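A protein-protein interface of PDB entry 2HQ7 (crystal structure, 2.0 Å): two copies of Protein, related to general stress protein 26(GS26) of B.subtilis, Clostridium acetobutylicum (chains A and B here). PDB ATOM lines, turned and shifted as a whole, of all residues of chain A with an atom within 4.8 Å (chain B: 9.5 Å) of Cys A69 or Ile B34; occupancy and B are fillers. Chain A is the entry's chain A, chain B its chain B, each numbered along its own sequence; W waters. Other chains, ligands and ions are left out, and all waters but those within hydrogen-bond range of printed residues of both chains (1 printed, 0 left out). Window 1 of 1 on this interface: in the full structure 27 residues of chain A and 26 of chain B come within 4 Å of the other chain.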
ATOM      1  N   MET A  22      28.827  10.921  18.260  1.00  0.00           N
ATOM      2  CA  MET A  22      28.705   9.560  18.723  1.00  0.00           C
ATOM      3  C   MET A  22      29.132   8.735  17.554  1.00  0.00           C
ATOM      4  O   MET A  22      28.677   8.980  16.438  1.00  0.00           O
ATOM      5  CB  MET A  22      27.255   9.198  19.070  1.00  0.00           C
ATOM      6  CG  MET A  22      26.619   9.942  20.246  1.00  0.00           C
ATOM      7  SD  MET A  22      27.855  10.249  21.717  1.00  0.00           S
ATOM      8  CE  MET A  22      28.211  12.166  21.515  1.00  0.00           C
ATOM      9  N   VAL A  23      29.986   7.758  17.787  1.00  0.00           N
ATOM     10  CA  VAL A  23      30.523   6.939  16.714  1.00  0.00           C
ATOM     11  C   VAL A  23      30.177   5.483  16.936  1.00  0.00           C
ATOM     12  O   VAL A  23      30.551   4.872  17.943  1.00  0.00           O
ATOM     13  CB  VAL A  23      32.072   7.120  16.553  1.00  0.00           C
ATOM     14  CG1 VAL A  23      32.660   6.245  15.457  1.00  0.00           C
ATOM     15  CG2 VAL A  23      32.425   8.584  16.272  1.00  0.00           C
ATOM     16  N   GLY A  24      29.461   4.930  15.972  1.00  0.00           N
ATOM     17  CA  GLY A  24      29.061   3.575  16.028  1.00  0.00           C
ATOM     18  C   GLY A  24      29.951   2.739  15.150  1.00  0.00           C
ATOM     19  O   GLY A  24      30.144   3.075  13.990  1.00  0.00           O
ATOM     20  N   ILE A  34      29.267   1.880  20.584  1.00  0.00           N
ATOM     21  CA  ILE A  34      29.255   3.343  20.417  1.00  0.00           C
ATOM     22  C   ILE A  34      30.254   4.018  21.369  1.00  0.00           C
ATOM     23  O   ILE A  34      30.368   3.610  22.513  1.00  0.00           O
ATOM     24  CB  ILE A  34      27.889   3.912  20.781  1.00  0.00           C
ATOM     25  CG1 ILE A  34      26.765   3.342  19.903  1.00  0.00           C
ATOM     26  CG2 ILE A  34      27.917   5.411  20.716  1.00  0.00           C
ATOM     27  CD1 ILE A  34      25.356   3.792  20.335  1.00  0.00           C
ATOM     28  N   LYS A  67      33.278  -0.127   8.433  1.00  0.00           N
ATOM     29  CA  LYS A  67      31.927   0.446   8.292  1.00  0.00           C
ATOM     30  C   LYS A  67      31.406   0.977   9.618  1.00  0.00           C
ATOM     31  O   LYS A  67      31.332   0.215  10.594  1.00  0.00           O
ATOM     32  CB  LYS A  67      30.971  -0.598   7.785  1.00  0.00           C
ATOM     33  CG  LYS A  67      31.230  -0.983   6.351  1.00  0.00           C
ATOM     34  CD  LYS A  67      30.181  -1.940   5.869  1.00  0.00           C
ATOM     35  CE  LYS A  67      30.467  -2.413   4.471  1.00  0.00           C
ATOM     36  NZ  LYS A  67      29.386  -3.382   4.027  1.00  0.00           N
ATOM     37  N   ILE A  68      31.043   2.261   9.632  1.00  0.00           N
ATOM     38  CA  ILE A  68      30.653   2.980  10.852  1.00  0.00           C
ATOM     39  C   ILE A  68      29.493   3.919  10.580  1.00  0.00           C
ATOM     40  O   ILE A  68      29.052   4.067   9.426  1.00  0.00           O
ATOM     41  CB  ILE A  68      31.814   3.801  11.445  1.00  0.00           C
ATOM     42  CG1 ILE A  68      32.167   5.013  10.612  1.00  0.00           C
ATOM     43  CG2 ILE A  68      33.085   2.984  11.620  1.00  0.00           C
ATOM     44  CD1 ILE A  68      32.730   6.067  11.529  1.00  0.00           C
ATOM     45  N   CYS A  69      28.964   4.500  11.646  1.00  0.00           N
ATOM     46  CA  CYS A  69      28.037   5.632  11.536  1.00  0.00           C
ATOM     47  C   CYS A  69      28.407   6.691  12.543  1.00  0.00           C
ATOM     48  O   CYS A  69      29.119   6.403  13.497  1.00  0.00           O
ATOM     49  CB  CYS A  69      26.618   5.163  11.709  1.00  0.00           C
ATOM     50  SG  CYS A  69      26.262   4.678  13.375  1.00  0.00           S
ATOM     51  N   LEU A  70      28.026   7.938  12.244  1.00  0.00           N
ATOM     52  CA  LEU A  70      28.115   9.078  13.131  1.00  0.00           C
ATOM     53  C   LEU A  70      26.712   9.490  13.510  1.00  0.00           C
ATOM     54  O   LEU A  70      25.827   9.496  12.665  1.00  0.00           O
ATOM     55  CB  LEU A  70      28.791  10.278  12.421  1.00  0.00           C
ATOM     56  CG  LEU A  70      30.301  10.437  12.536  1.00  0.00           C
ATOM     57  CD1 LEU A  70      30.971   9.167  12.125  1.00  0.00           C
ATOM     58  CD2 LEU A  70      30.849  11.678  11.752  1.00  0.00           C
ATOM     59  N   TYR A  71      26.500   9.907  14.747  1.00  0.00           N
ATOM     60  CA  TYR A  71      25.219  10.449  15.127  1.00  0.00           C
ATOM     61  C   TYR A  71      25.432  11.777  15.843  1.00  0.00           C
ATOM     62  O   TYR A  71      26.238  11.845  16.752  1.00  0.00           O
ATOM     63  CB  TYR A  71      24.497   9.496  16.067  1.00  0.00           C
ATOM     64  CG  TYR A  71      23.055   9.892  16.337  1.00  0.00           C
ATOM     65  CD1 TYR A  71      22.043   9.463  15.493  1.00  0.00           C
ATOM     66  CD2 TYR A  71      22.701  10.615  17.447  1.00  0.00           C
ATOM     67  CE1 TYR A  71      20.741   9.793  15.721  1.00  0.00           C
ATOM     68  CE2 TYR A  71      21.379  10.974  17.673  1.00  0.00           C
ATOM     69  CZ  TYR A  71      20.405  10.534  16.814  1.00  0.00           C
ATOM     70  OH  TYR A  71      19.079  10.866  17.014  1.00  0.00           O
ATOM     71  N   MET A  82      22.113  11.117  11.429  1.00  0.00           N
ATOM     72  CA  MET A  82      22.942   9.963  11.393  1.00  0.00           C
ATOM     73  C   MET A  82      23.597   9.932  10.037  1.00  0.00           C
ATOM     74  O   MET A  82      22.910  10.036   9.031  1.00  0.00           O
ATOM     75  CB  MET A  82      22.094   8.706  11.543  1.00  0.00           C
ATOM     76  CG  MET A  82      22.834   7.593  12.169  1.00  0.00           C
ATOM     77  SD  MET A  82      22.619   5.967  11.217  1.00  0.00           S
ATOM     78  CE  MET A  82      20.747   5.887  10.810  1.00  0.00           C
ATOM     79  N   LEU A  83      24.913   9.808  10.011  1.00  0.00           N
ATOM     80  CA  LEU A  83      25.621   9.539   8.758  1.00  0.00           C
ATOM     81  C   LEU A  83      26.235   8.158   8.796  1.00  0.00           C
ATOM     82  O   LEU A  83      26.721   7.688   9.819  1.00  0.00           O
ATOM     83  CB  LEU A  83      26.675  10.600   8.497  1.00  0.00           C
ATOM     84  CG  LEU A  83      26.236  12.072   8.569  1.00  0.00           C
ATOM     85  CD1 LEU A  83      27.476  12.976   8.497  1.00  0.00           C
ATOM     86  CD2 LEU A  83      25.250  12.489   7.466  1.00  0.00           C
ATOM     87  N   VAL A  84      26.204   7.502   7.653  1.00  0.00           N
ATOM     88  CA  VAL A  84      26.758   6.186   7.518  1.00  0.00           C
ATOM     89  C   VAL A  84      27.827   6.210   6.435  1.00  0.00           C
ATOM     90  O   VAL A  84      27.655   6.841   5.415  1.00  0.00           O
ATOM     91  CB  VAL A  84      25.633   5.227   7.144  1.00  0.00           C
ATOM     92  CG1 VAL A  84      26.180   3.922   6.731  1.00  0.00           C
ATOM     93  CG2 VAL A  84      24.652   5.068   8.332  1.00  0.00           C
ATOM     94  N   TYR A 130      16.418  12.693  11.468  1.00  0.00           N
ATOM     95  CA  TYR A 130      15.322  12.315  12.353  1.00  0.00           C
ATOM     96  C   TYR A 130      14.707  13.556  12.937  1.00  0.00           C
ATOM     97  O   TYR A 130      15.407  14.371  13.564  1.00  0.00           O
ATOM     98  CB  TYR A 130      15.814  11.486  13.516  1.00  0.00           C
ATOM     99  CG  TYR A 130      16.408  10.173  13.119  1.00  0.00           C
ATOM    100  CD1 TYR A 130      15.604   9.045  12.973  1.00  0.00           C
ATOM    101  CD2 TYR A 130      17.787  10.043  12.894  1.00  0.00           C
ATOM    102  CE1 TYR A 130      16.154   7.811  12.613  1.00  0.00           C
ATOM    103  CE2 TYR A 130      18.345   8.820  12.535  1.00  0.00           C
ATOM    104  CZ  TYR A 130      17.525   7.709  12.401  1.00  0.00           C
ATOM    105  OH  TYR A 130      18.072   6.494  12.043  1.00  0.00           O
ATOM    106  N   ILE B  20      16.386  10.075  27.381  1.00  0.00           N
ATOM    107  CA  ILE B  20      16.778   9.713  26.008  1.00  0.00           C
ATOM    108  C   ILE B  20      17.987   8.813  26.020  1.00  0.00           C
ATOM    109  O   ILE B  20      18.953   9.084  26.706  1.00  0.00           O
ATOM    110  CB  ILE B  20      17.140  10.959  25.153  1.00  0.00           C
ATOM    111  CG1 ILE B  20      16.066  12.042  25.278  1.00  0.00           C
ATOM    112  CG2 ILE B  20      17.290  10.586  23.681  1.00  0.00           C
ATOM    113  CD1 ILE B  20      14.666  11.544  24.924  1.00  0.00           C
ATOM    114  N   VAL B  21      17.938   7.733  25.262  1.00  0.00           N
ATOM    115  CA  VAL B  21      19.076   6.852  25.173  1.00  0.00           C
ATOM    116  C   VAL B  21      19.384   6.634  23.710  1.00  0.00           C
ATOM    117  O   VAL B  21      18.473   6.492  22.882  1.00  0.00           O
ATOM    118  CB  VAL B  21      18.831   5.479  25.884  1.00  0.00           C
ATOM    119  CG1 VAL B  21      17.788   4.734  25.227  1.00  0.00           C
ATOM    120  CG2 VAL B  21      20.076   4.650  25.867  1.00  0.00           C
ATOM    121  N   MET B  22      20.672   6.552  23.412  1.00  0.00           N
ATOM    122  CA  MET B  22      21.141   6.320  22.051  1.00  0.00           C
ATOM    123  C   MET B  22      21.227   4.824  21.867  1.00  0.00           C
ATOM    124  O   MET B  22      21.868   4.138  22.680  1.00  0.00           O
ATOM    125  CB  MET B  22      22.534   6.834  21.879  1.00  0.00           C
ATOM    126  CG  MET B  22      22.868   8.167  22.454  1.00  0.00           C
ATOM    127  SD  MET B  22      22.708   9.303  21.002  1.00  0.00           S
ATOM    128  CE  MET B  22      20.821   9.676  21.342  1.00  0.00           C
ATOM    129  N   VAL B  23      20.639   4.300  20.814  1.00  0.00           N
ATOM    130  CA  VAL B  23      20.574   2.855  20.656  1.00  0.00           C
ATOM    131  C   VAL B  23      21.277   2.469  19.369  1.00  0.00           C
ATOM    132  O   VAL B  23      20.847   2.872  18.272  1.00  0.00           O
ATOM    133  CB  VAL B  23      19.141   2.371  20.559  1.00  0.00           C
ATOM    134  CG1 VAL B  23      19.126   0.877  20.315  1.00  0.00           C
ATOM    135  CG2 VAL B  23      18.369   2.758  21.776  1.00  0.00           C
ATOM    136  N   GLY B  24      22.327   1.664  19.494  1.00  0.00           N
ATOM    137  CA  GLY B  24      23.037   1.160  18.347  1.00  0.00           C
ATOM    138  C   GLY B  24      22.517  -0.200  17.892  1.00  0.00           C
ATOM    139  O   GLY B  24      22.340  -1.083  18.694  1.00  0.00           O
ATOM    140  N   THR B  25      22.275  -0.339  16.597  1.00  0.00           N
ATOM    141  CA  THR B  25      21.782  -1.554  16.015  1.00  0.00           C
ATOM    142  C   THR B  25      22.599  -1.895  14.768  1.00  0.00           C
ATOM    143  O   THR B  25      23.333  -1.073  14.250  1.00  0.00           O
ATOM    144  CB  THR B  25      20.296  -1.432  15.593  1.00  0.00           C
ATOM    145  OG1 THR B  25      20.129  -0.287  14.747  1.00  0.00           O
ATOM    146  CG2 THR B  25      19.389  -1.335  16.762  1.00  0.00           C
ATOM    147  N   ASN B  26      22.438  -3.121  14.309  1.00  0.00           N
ATOM    148  CA  ASN B  26      23.082  -3.592  13.090  1.00  0.00           C
ATOM    149  C   ASN B  26      22.196  -3.284  11.906  1.00  0.00           C
ATOM    150  O   ASN B  26      21.175  -3.921  11.741  1.00  0.00           O
ATOM    151  CB  ASN B  26      23.333  -5.070  13.170  1.00  0.00           C
ATOM    152  CG  ASN B  26      24.381  -5.423  14.197  1.00  0.00           C
ATOM    153  OD1 ASN B  26      24.170  -6.277  15.045  1.00  0.00           O
ATOM    154  ND2 ASN B  26      25.504  -4.765  14.129  1.00  0.00           N
ATOM    155  N   GLY B  27      22.568  -2.269  11.130  1.00  0.00           N
ATOM    156  CA  GLY B  27      21.761  -1.812  10.012  1.00  0.00           C
ATOM    157  C   GLY B  27      22.028  -2.566   8.722  1.00  0.00           C
ATOM    158  O   GLY B  27      22.792  -3.538   8.691  1.00  0.00           O
ATOM    159  N   GLU B  28      21.369  -2.124   7.657  1.00  0.00           N
ATOM    160  CA  GLU B  28      21.521  -2.759   6.345  1.00  0.00           C
ATOM    161  C   GLU B  28      22.945  -2.618   5.856  1.00  0.00           C
ATOM    162  O   GLU B  28      23.632  -1.619   6.162  1.00  0.00           O
ATOM    163  CB  GLU B  28      20.564  -2.135   5.311  1.00  0.00           C
ATOM    164  CG  GLU B  28      19.083  -2.414   5.543  1.00  0.00           C
ATOM    165  N   GLY B  30      25.705  -4.017   6.557  1.00  0.00           N
ATOM    166  CA  GLY B  30      26.822  -4.188   7.456  1.00  0.00           C
ATOM    167  C   GLY B  30      27.279  -2.920   8.162  1.00  0.00           C
ATOM    168  O   GLY B  30      28.329  -2.933   8.800  1.00  0.00           O
ATOM    169  N   TYR B  31      26.494  -1.849   8.058  1.00  0.00           N
ATOM    170  CA  TYR B  31      26.753  -0.588   8.763  1.00  0.00           C
ATOM    171  C   TYR B  31      25.993  -0.508  10.087  1.00  0.00           C
ATOM    172  O   TYR B  31      24.817  -0.886  10.152  1.00  0.00           O
ATOM    173  CB  TYR B  31      26.307   0.580   7.903  1.00  0.00           C
ATOM    174  CG  TYR B  31      27.070   0.749   6.619  1.00  0.00           C
ATOM    175  CD1 TYR B  31      26.670   0.103   5.446  1.00  0.00           C
ATOM    176  CD2 TYR B  31      28.198   1.552   6.576  1.00  0.00           C
ATOM    177  CE1 TYR B  31      27.387   0.270   4.255  1.00  0.00           C
ATOM    178  CE2 TYR B  31      28.902   1.733   5.412  1.00  0.00           C
ATOM    179  CZ  TYR B  31      28.506   1.091   4.251  1.00  0.00           C
ATOM    180  OH  TYR B  31      29.268   1.294   3.111  1.00  0.00           O
ATOM    181  N   PRO B  32      26.649  -0.004  11.160  1.00  0.00           N
ATOM    182  CA  PRO B  32      25.876   0.214  12.358  1.00  0.00           C
ATOM    183  C   PRO B  32      24.979   1.430  12.184  1.00  0.00           C
ATOM    184  O   PRO B  32      25.189   2.262  11.308  1.00  0.00           O
ATOM    185  CB  PRO B  32      26.928   0.457  13.431  1.00  0.00           C
ATOM    186  CG  PRO B  32      28.213   0.282  12.791  1.00  0.00           C
ATOM    187  CD  PRO B  32      28.053   0.356  11.352  1.00  0.00           C
ATOM    188  N   ASN B  33      23.926   1.472  12.957  1.00  0.00           N
ATOM    189  CA  ASN B  33      23.005   2.569  12.892  1.00  0.00           C
ATOM    190  C   ASN B  33      22.784   2.962  14.333  1.00  0.00           C
ATOM    191  O   ASN B  33      22.867   2.134  15.209  1.00  0.00           O
ATOM    192  CB  ASN B  33      21.671   2.168  12.279  1.00  0.00           C
ATOM    193  CG  ASN B  33      21.709   1.939  10.789  1.00  0.00           C
ATOM    194  OD1 ASN B  33      20.652   1.631  10.229  1.00  0.00           O
ATOM    195  ND2 ASN B  33      22.877   2.074  10.130  1.00  0.00           N
ATOM    196  N   ILE B  34      22.572   4.243  14.559  1.00  0.00           N
ATOM    197  CA  ILE B  34      22.254   4.759  15.869  1.00  0.00           C
ATOM    198  C   ILE B  34      20.969   5.549  15.758  1.00  0.00           C
ATOM    199  O   ILE B  34      20.832   6.380  14.847  1.00  0.00           O
ATOM    200  CB  ILE B  34      23.357   5.709  16.404  1.00  0.00           C
ATOM    201  CG1 ILE B  34      24.686   4.969  16.554  1.00  0.00           C
ATOM    202  CG2 ILE B  34      22.938   6.311  17.740  1.00  0.00           C
ATOM    203  CD1 ILE B  34      25.923   5.890  16.907  1.00  0.00           C
ATOM    204  N   LYS B  35      20.053   5.293  16.696  1.00  0.00           N
ATOM    205  CA  LYS B  35      18.823   6.063  16.878  1.00  0.00           C
ATOM    206  C   LYS B  35      18.613   6.438  18.333  1.00  0.00           C
ATOM    207  O   LYS B  35      18.961   5.661  19.222  1.00  0.00           O
ATOM    208  CB  LYS B  35      17.628   5.219  16.443  1.00  0.00           C
ATOM    209  CG  LYS B  35      16.396   6.016  16.192  1.00  0.00           C
ATOM    210  CD  LYS B  35      15.344   5.130  15.564  1.00  0.00           C
ATOM    211  CE  LYS B  35      14.048   5.869  15.312  1.00  0.00           C
ATOM    212  NZ  LYS B  35      13.131   5.006  14.499  1.00  0.00           N
ATOM    213  N   ALA B  36      18.036   7.620  18.566  1.00  0.00           N
ATOM    214  CA  ALA B  36      17.562   8.024  19.897  1.00  0.00           C
ATOM    215  C   ALA B  36      16.240   7.313  20.247  1.00  0.00           C
ATOM    216  O   ALA B  36      15.363   7.136  19.401  1.00  0.00           O
ATOM    217  CB  ALA B  36      17.406   9.546  19.991  1.00  0.00           C
ATOM    218  N   MET B  37      16.157   6.805  21.469  1.00  0.00           N
ATOM    219  CA  MET B  37      14.938   6.180  21.963  1.00  0.00           C
ATOM    220  C   MET B  37      14.636   6.697  23.336  1.00  0.00           C
ATOM    221  O   MET B  37      15.463   7.358  23.943  1.00  0.00           O
ATOM    222  CB  MET B  37      15.082   4.667  21.991  1.00  0.00           C
ATOM    223  CG  MET B  37      15.020   4.065  20.627  1.00  0.00           C
ATOM    224  SD  MET B  37      14.899   2.128  20.675  1.00  0.00           S
ATOM    225  CE  MET B  37      13.408   1.845  21.892  1.00  0.00           C
ATOM    226  N   THR B  52      10.017   3.492  21.168  1.00  0.00           N
ATOM    227  CA  THR B  52      10.306   4.098  19.885  1.00  0.00           C
ATOM    228  C   THR B  52       9.093   3.963  18.977  1.00  0.00           C
ATOM    229  O   THR B  52       8.133   3.222  19.277  1.00  0.00           O
ATOM    230  CB  THR B  52      11.570   3.481  19.246  1.00  0.00           C
ATOM    231  OG1 THR B  52      12.081   4.355  18.229  1.00  0.00           O
ATOM    232  CG2 THR B  52      11.289   2.066  18.683  1.00  0.00           C
ATOM    233  N   MET B  58      12.768  -1.121  11.304  1.00  0.00           N
ATOM    234  CA  MET B  58      13.410  -1.395  12.582  1.00  0.00           C
ATOM    235  C   MET B  58      12.959  -2.738  13.131  1.00  0.00           C
ATOM    236  O   MET B  58      13.765  -3.510  13.611  1.00  0.00           O
ATOM    237  CB  MET B  58      13.086  -0.286  13.600  1.00  0.00           C
ATOM    238  CG  MET B  58      13.672  -0.463  14.988  1.00  0.00           C
ATOM    239  SD  MET B  58      15.661  -0.482  15.057  1.00  0.00           S
ATOM    240  CE  MET B  58      16.046  -2.165  14.170  1.00  0.00           C
ATOM    241  N   ARG B  61      14.412  -5.645  11.202  1.00  0.00           N
ATOM    242  CA  ARG B  61      15.828  -5.697  11.556  1.00  0.00           C
ATOM    243  C   ARG B  61      16.070  -6.311  12.930  1.00  0.00           C
ATOM    244  O   ARG B  61      16.957  -7.147  13.088  1.00  0.00           O
ATOM    245  CB  ARG B  61      16.463  -4.298  11.530  1.00  0.00           C
ATOM    246  CG  ARG B  61      17.884  -4.208  12.233  1.00  0.00           C
ATOM    247  CD  ARG B  61      18.450  -2.770  12.367  1.00  0.00           C
ATOM    248  NE  ARG B  61      18.145  -2.014  11.157  1.00  0.00           N
ATOM    249  CZ  ARG B  61      18.217  -0.698  11.040  1.00  0.00           C
ATOM    250  NH1 ARG B  61      18.636   0.069  12.047  1.00  0.00           N
ATOM    251  NH2 ARG B  61      17.872  -0.148   9.888  1.00  0.00           N
ATOM    252  N   ILE B  68      22.430  -5.320  20.248  1.00  0.00           N
ATOM    253  CA  ILE B  68      22.391  -3.897  20.245  1.00  0.00           C
ATOM    254  C   ILE B  68      23.333  -3.362  21.298  1.00  0.00           C
ATOM    255  O   ILE B  68      23.896  -4.100  22.135  1.00  0.00           O
ATOM    256  CB  ILE B  68      20.953  -3.324  20.464  1.00  0.00           C
ATOM    257  CG1 ILE B  68      20.464  -3.545  21.887  1.00  0.00           C
ATOM    258  CG2 ILE B  68      19.946  -3.848  19.447  1.00  0.00           C
ATOM    259  CD1 ILE B  68      19.497  -2.452  22.321  1.00  0.00           C
ATOM    260  N   CYS B  69      23.470  -2.058  21.294  1.00  0.00           N
ATOM    261  CA  CYS B  69      24.077  -1.415  22.426  1.00  0.00           C
ATOM    262  C   CYS B  69      23.351  -0.131  22.740  1.00  0.00           C
ATOM    263  O   CYS B  69      22.681   0.463  21.888  1.00  0.00           O
ATOM    264  CB  CYS B  69      25.549  -1.185  22.193  1.00  0.00           C
ATOM    265  SG  CYS B  69      25.903   0.241  21.239  1.00  0.00           S
ATOM    266  N   LEU B  70      23.423   0.250  23.991  1.00  0.00           N
ATOM    267  CA  LEU B  70      22.893   1.559  24.464  1.00  0.00           C
ATOM    268  C   LEU B  70      24.032   2.467  24.829  1.00  0.00           C
ATOM    269  O   LEU B  70      25.058   2.007  25.355  1.00  0.00           O
ATOM    270  CB  LEU B  70      22.026   1.380  25.716  1.00  0.00           C
ATOM    271  CG  LEU B  70      20.799   0.453  25.687  1.00  0.00           C
ATOM    272  CD1 LEU B  70      19.926   0.671  26.955  1.00  0.00           C
ATOM    273  CD2 LEU B  70      19.989   0.738  24.504  1.00  0.00           C
ATOM    274  N   TYR B  71      23.862   3.765  24.614  1.00  0.00           N
ATOM    275  CA  TYR B  71      24.883   4.737  25.045  1.00  0.00           C
ATOM    276  C   TYR B  71      24.250   5.932  25.748  1.00  0.00           C
ATOM    277  O   TYR B  71      23.247   6.465  25.282  1.00  0.00           O
ATOM    278  CB  TYR B  71      25.707   5.207  23.841  1.00  0.00           C
ATOM    279  CG  TYR B  71      26.946   5.979  24.203  1.00  0.00           C
ATOM    280  CD1 TYR B  71      28.121   5.317  24.532  1.00  0.00           C
ATOM    281  CD2 TYR B  71      26.942   7.350  24.237  1.00  0.00           C
ATOM    282  CE1 TYR B  71      29.266   6.015  24.883  1.00  0.00           C
ATOM    283  CE2 TYR B  71      28.094   8.055  24.595  1.00  0.00           C
ATOM    284  CZ  TYR B  71      29.240   7.367  24.912  1.00  0.00           C
ATOM    285  OH  TYR B  71      30.364   8.069  25.266  1.00  0.00           O
ATOM    286  N   PHE B  72      24.859   6.351  26.854  1.00  0.00           N
ATOM    287  CA  PHE B  72      24.405   7.481  27.637  1.00  0.00           C
ATOM    288  C   PHE B  72      25.563   8.400  27.750  1.00  0.00           C
ATOM    289  O   PHE B  72      26.662   7.951  28.037  1.00  0.00           O
ATOM    290  CB  PHE B  72      24.032   7.058  29.061  1.00  0.00           C
ATOM    291  CG  PHE B  72      23.061   5.944  29.117  1.00  0.00           C
ATOM    292  CD1 PHE B  72      23.495   4.640  28.972  1.00  0.00           C
ATOM    293  CD2 PHE B  72      21.698   6.193  29.271  1.00  0.00           C
ATOM    294  CE1 PHE B  72      22.611   3.605  29.006  1.00  0.00           C
ATOM    295  CE2 PHE B  72      20.801   5.134  29.287  1.00  0.00           C
ATOM    296  CZ  PHE B  72      21.271   3.846  29.166  1.00  0.00           C
HETATM  297  O   HOH W   1      17.240   9.281  16.224  1.00  0.00           O
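No residue of chain B comes within 4 Å of Val A23. Gly A24 touches just these residues of chain B: Pro B32 and Ile B34. Of the printed residues of chain B, Lys A67 touches Gly B30, Tyr B31 and Pro B32. Ile A68 touches just these residues of chain B: Tyr B31 and Pro B32. Of chain B, only Pro B32, Asn B33 and Ile B34 come within 4 Å of Cys A69. Printed residues of chain B within 4 Å of Met A82: Asn B33 and Ile B34. Of the printed residues of chain A, Ile B34 touches Gly A24 (3.8 Å), Cys A69 (3.6 Å), Tyr A71 (3.4 Å), Met A82 (3.6 Å) and Tyr A130 (3.9 Å). Arg B61 touches none of the printed residues of chain A. The nearest residue of chain B that does not touch Cys A69 is Tyr B31 (5.9 Å). The nearest printed residue of chain A that does not touch Ile B34 is Ile A34 (4.02 Å).
Met A22 touches Tyr B71, and with the chains exchanged Tyr A71 touches Met B22. Gly A24 touches Ile B34, and with the chains exchanged Ile A34 touches Gly B24. Ile A34 touches Cys B69, and with the chains exchanged Cys A69 touches Ile B34. Ile A34 touches Tyr B71, and with the chains exchanged Tyr A71 touches Ile B34.
The backbone NH (N) of Ile A34 lies close to the side-chain sulfur (SG) of Cys B69 (3.8 Å). The side-chain sulfur (SG) of Cys A69 lies close to the backbone carbonyl oxygen (O) of Pro B32 (3.4 Å). SD of Met A82 sits at hydrogen-bond distance from N of Ile B34.
Water W1 bridges the side-chain hydroxyl (OH) of Tyr A71 and the backbone NH (N) of Ala B36.
N of Tyr A71 sits at hydrogen-bond distance from O of Met A22, at 2.9 Å. O of Met B22 sits at hydrogen-bond distance from N of Tyr B71, 2.8 Å away. N of Val B23 is in hydrogen-bond range of O of Lys B35. The backbone NH (N) of Gly B24 lies within hydrogen-bond range of the backbone carbonyl oxygen (O) of Cys B69, 2.7 Å away. O of Asn B33 lies within hydrogen-bond range of N of Thr B25 (2.9 Å). The guanidinium group (NH1) of Arg B61 sits at hydrogen-bond distance from the side-chain amide oxygen (OD1) of Asn B33, at 3.1 Å.
Hydrophobic or aromatic side chains of chain A that line the printed part of chain B: Met A22, Ile A34, Tyr A71, Met A82, Val A84 and Tyr A130. Along chain A the printed residues that touch a printed residue of chain B span positions 22 to 130. Of the 25 printed residues of chain B, 11 touch a printed residue of chain A. Printed residues of chain B that touch a printed residue of chain A: Met B22, Gly B24, Gly B30, Tyr B31, Pro B32, Asn B33, Ile B34, Lys B35, Ala B36, Cys B69 and Tyr B71. Hydrophobic or aromatic side chains of chain B within 4 Å of the printed part of chain A: Met B22, Tyr B31, Pro B32, Ile B34, Ala B36 and Tyr B71. Among the printed residues, no Asp or Glu carboxylate lies within 4 Å of a Lys or Arg side-chain nitrogen of the other chain.
Among the printed residues, pairs that only touch across the chains: Met A22 with Tyr B71, Gly A24 with Pro B32, Gly A24 with Ile B34, Ile A34 with Gly B24, Ile A34 with Tyr B71, Lys A67 with Gly B30, Lys A67 with Tyr B31, Lys A67 with Pro B32, Ile A68 with Tyr B31, Ile A68 with Pro B32, Cys A69 with Asn B33, Cys A69 with Ile B34, Tyr A71 with Met B22, Tyr A71 with Ile B34, Tyr A71 with Ala B36, Met A82 with Asn B33, Val A84 with Tyr B31, Val A84 with Asn B33, Tyr A130 with Ile B34 and Tyr A130 with Lys B35.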
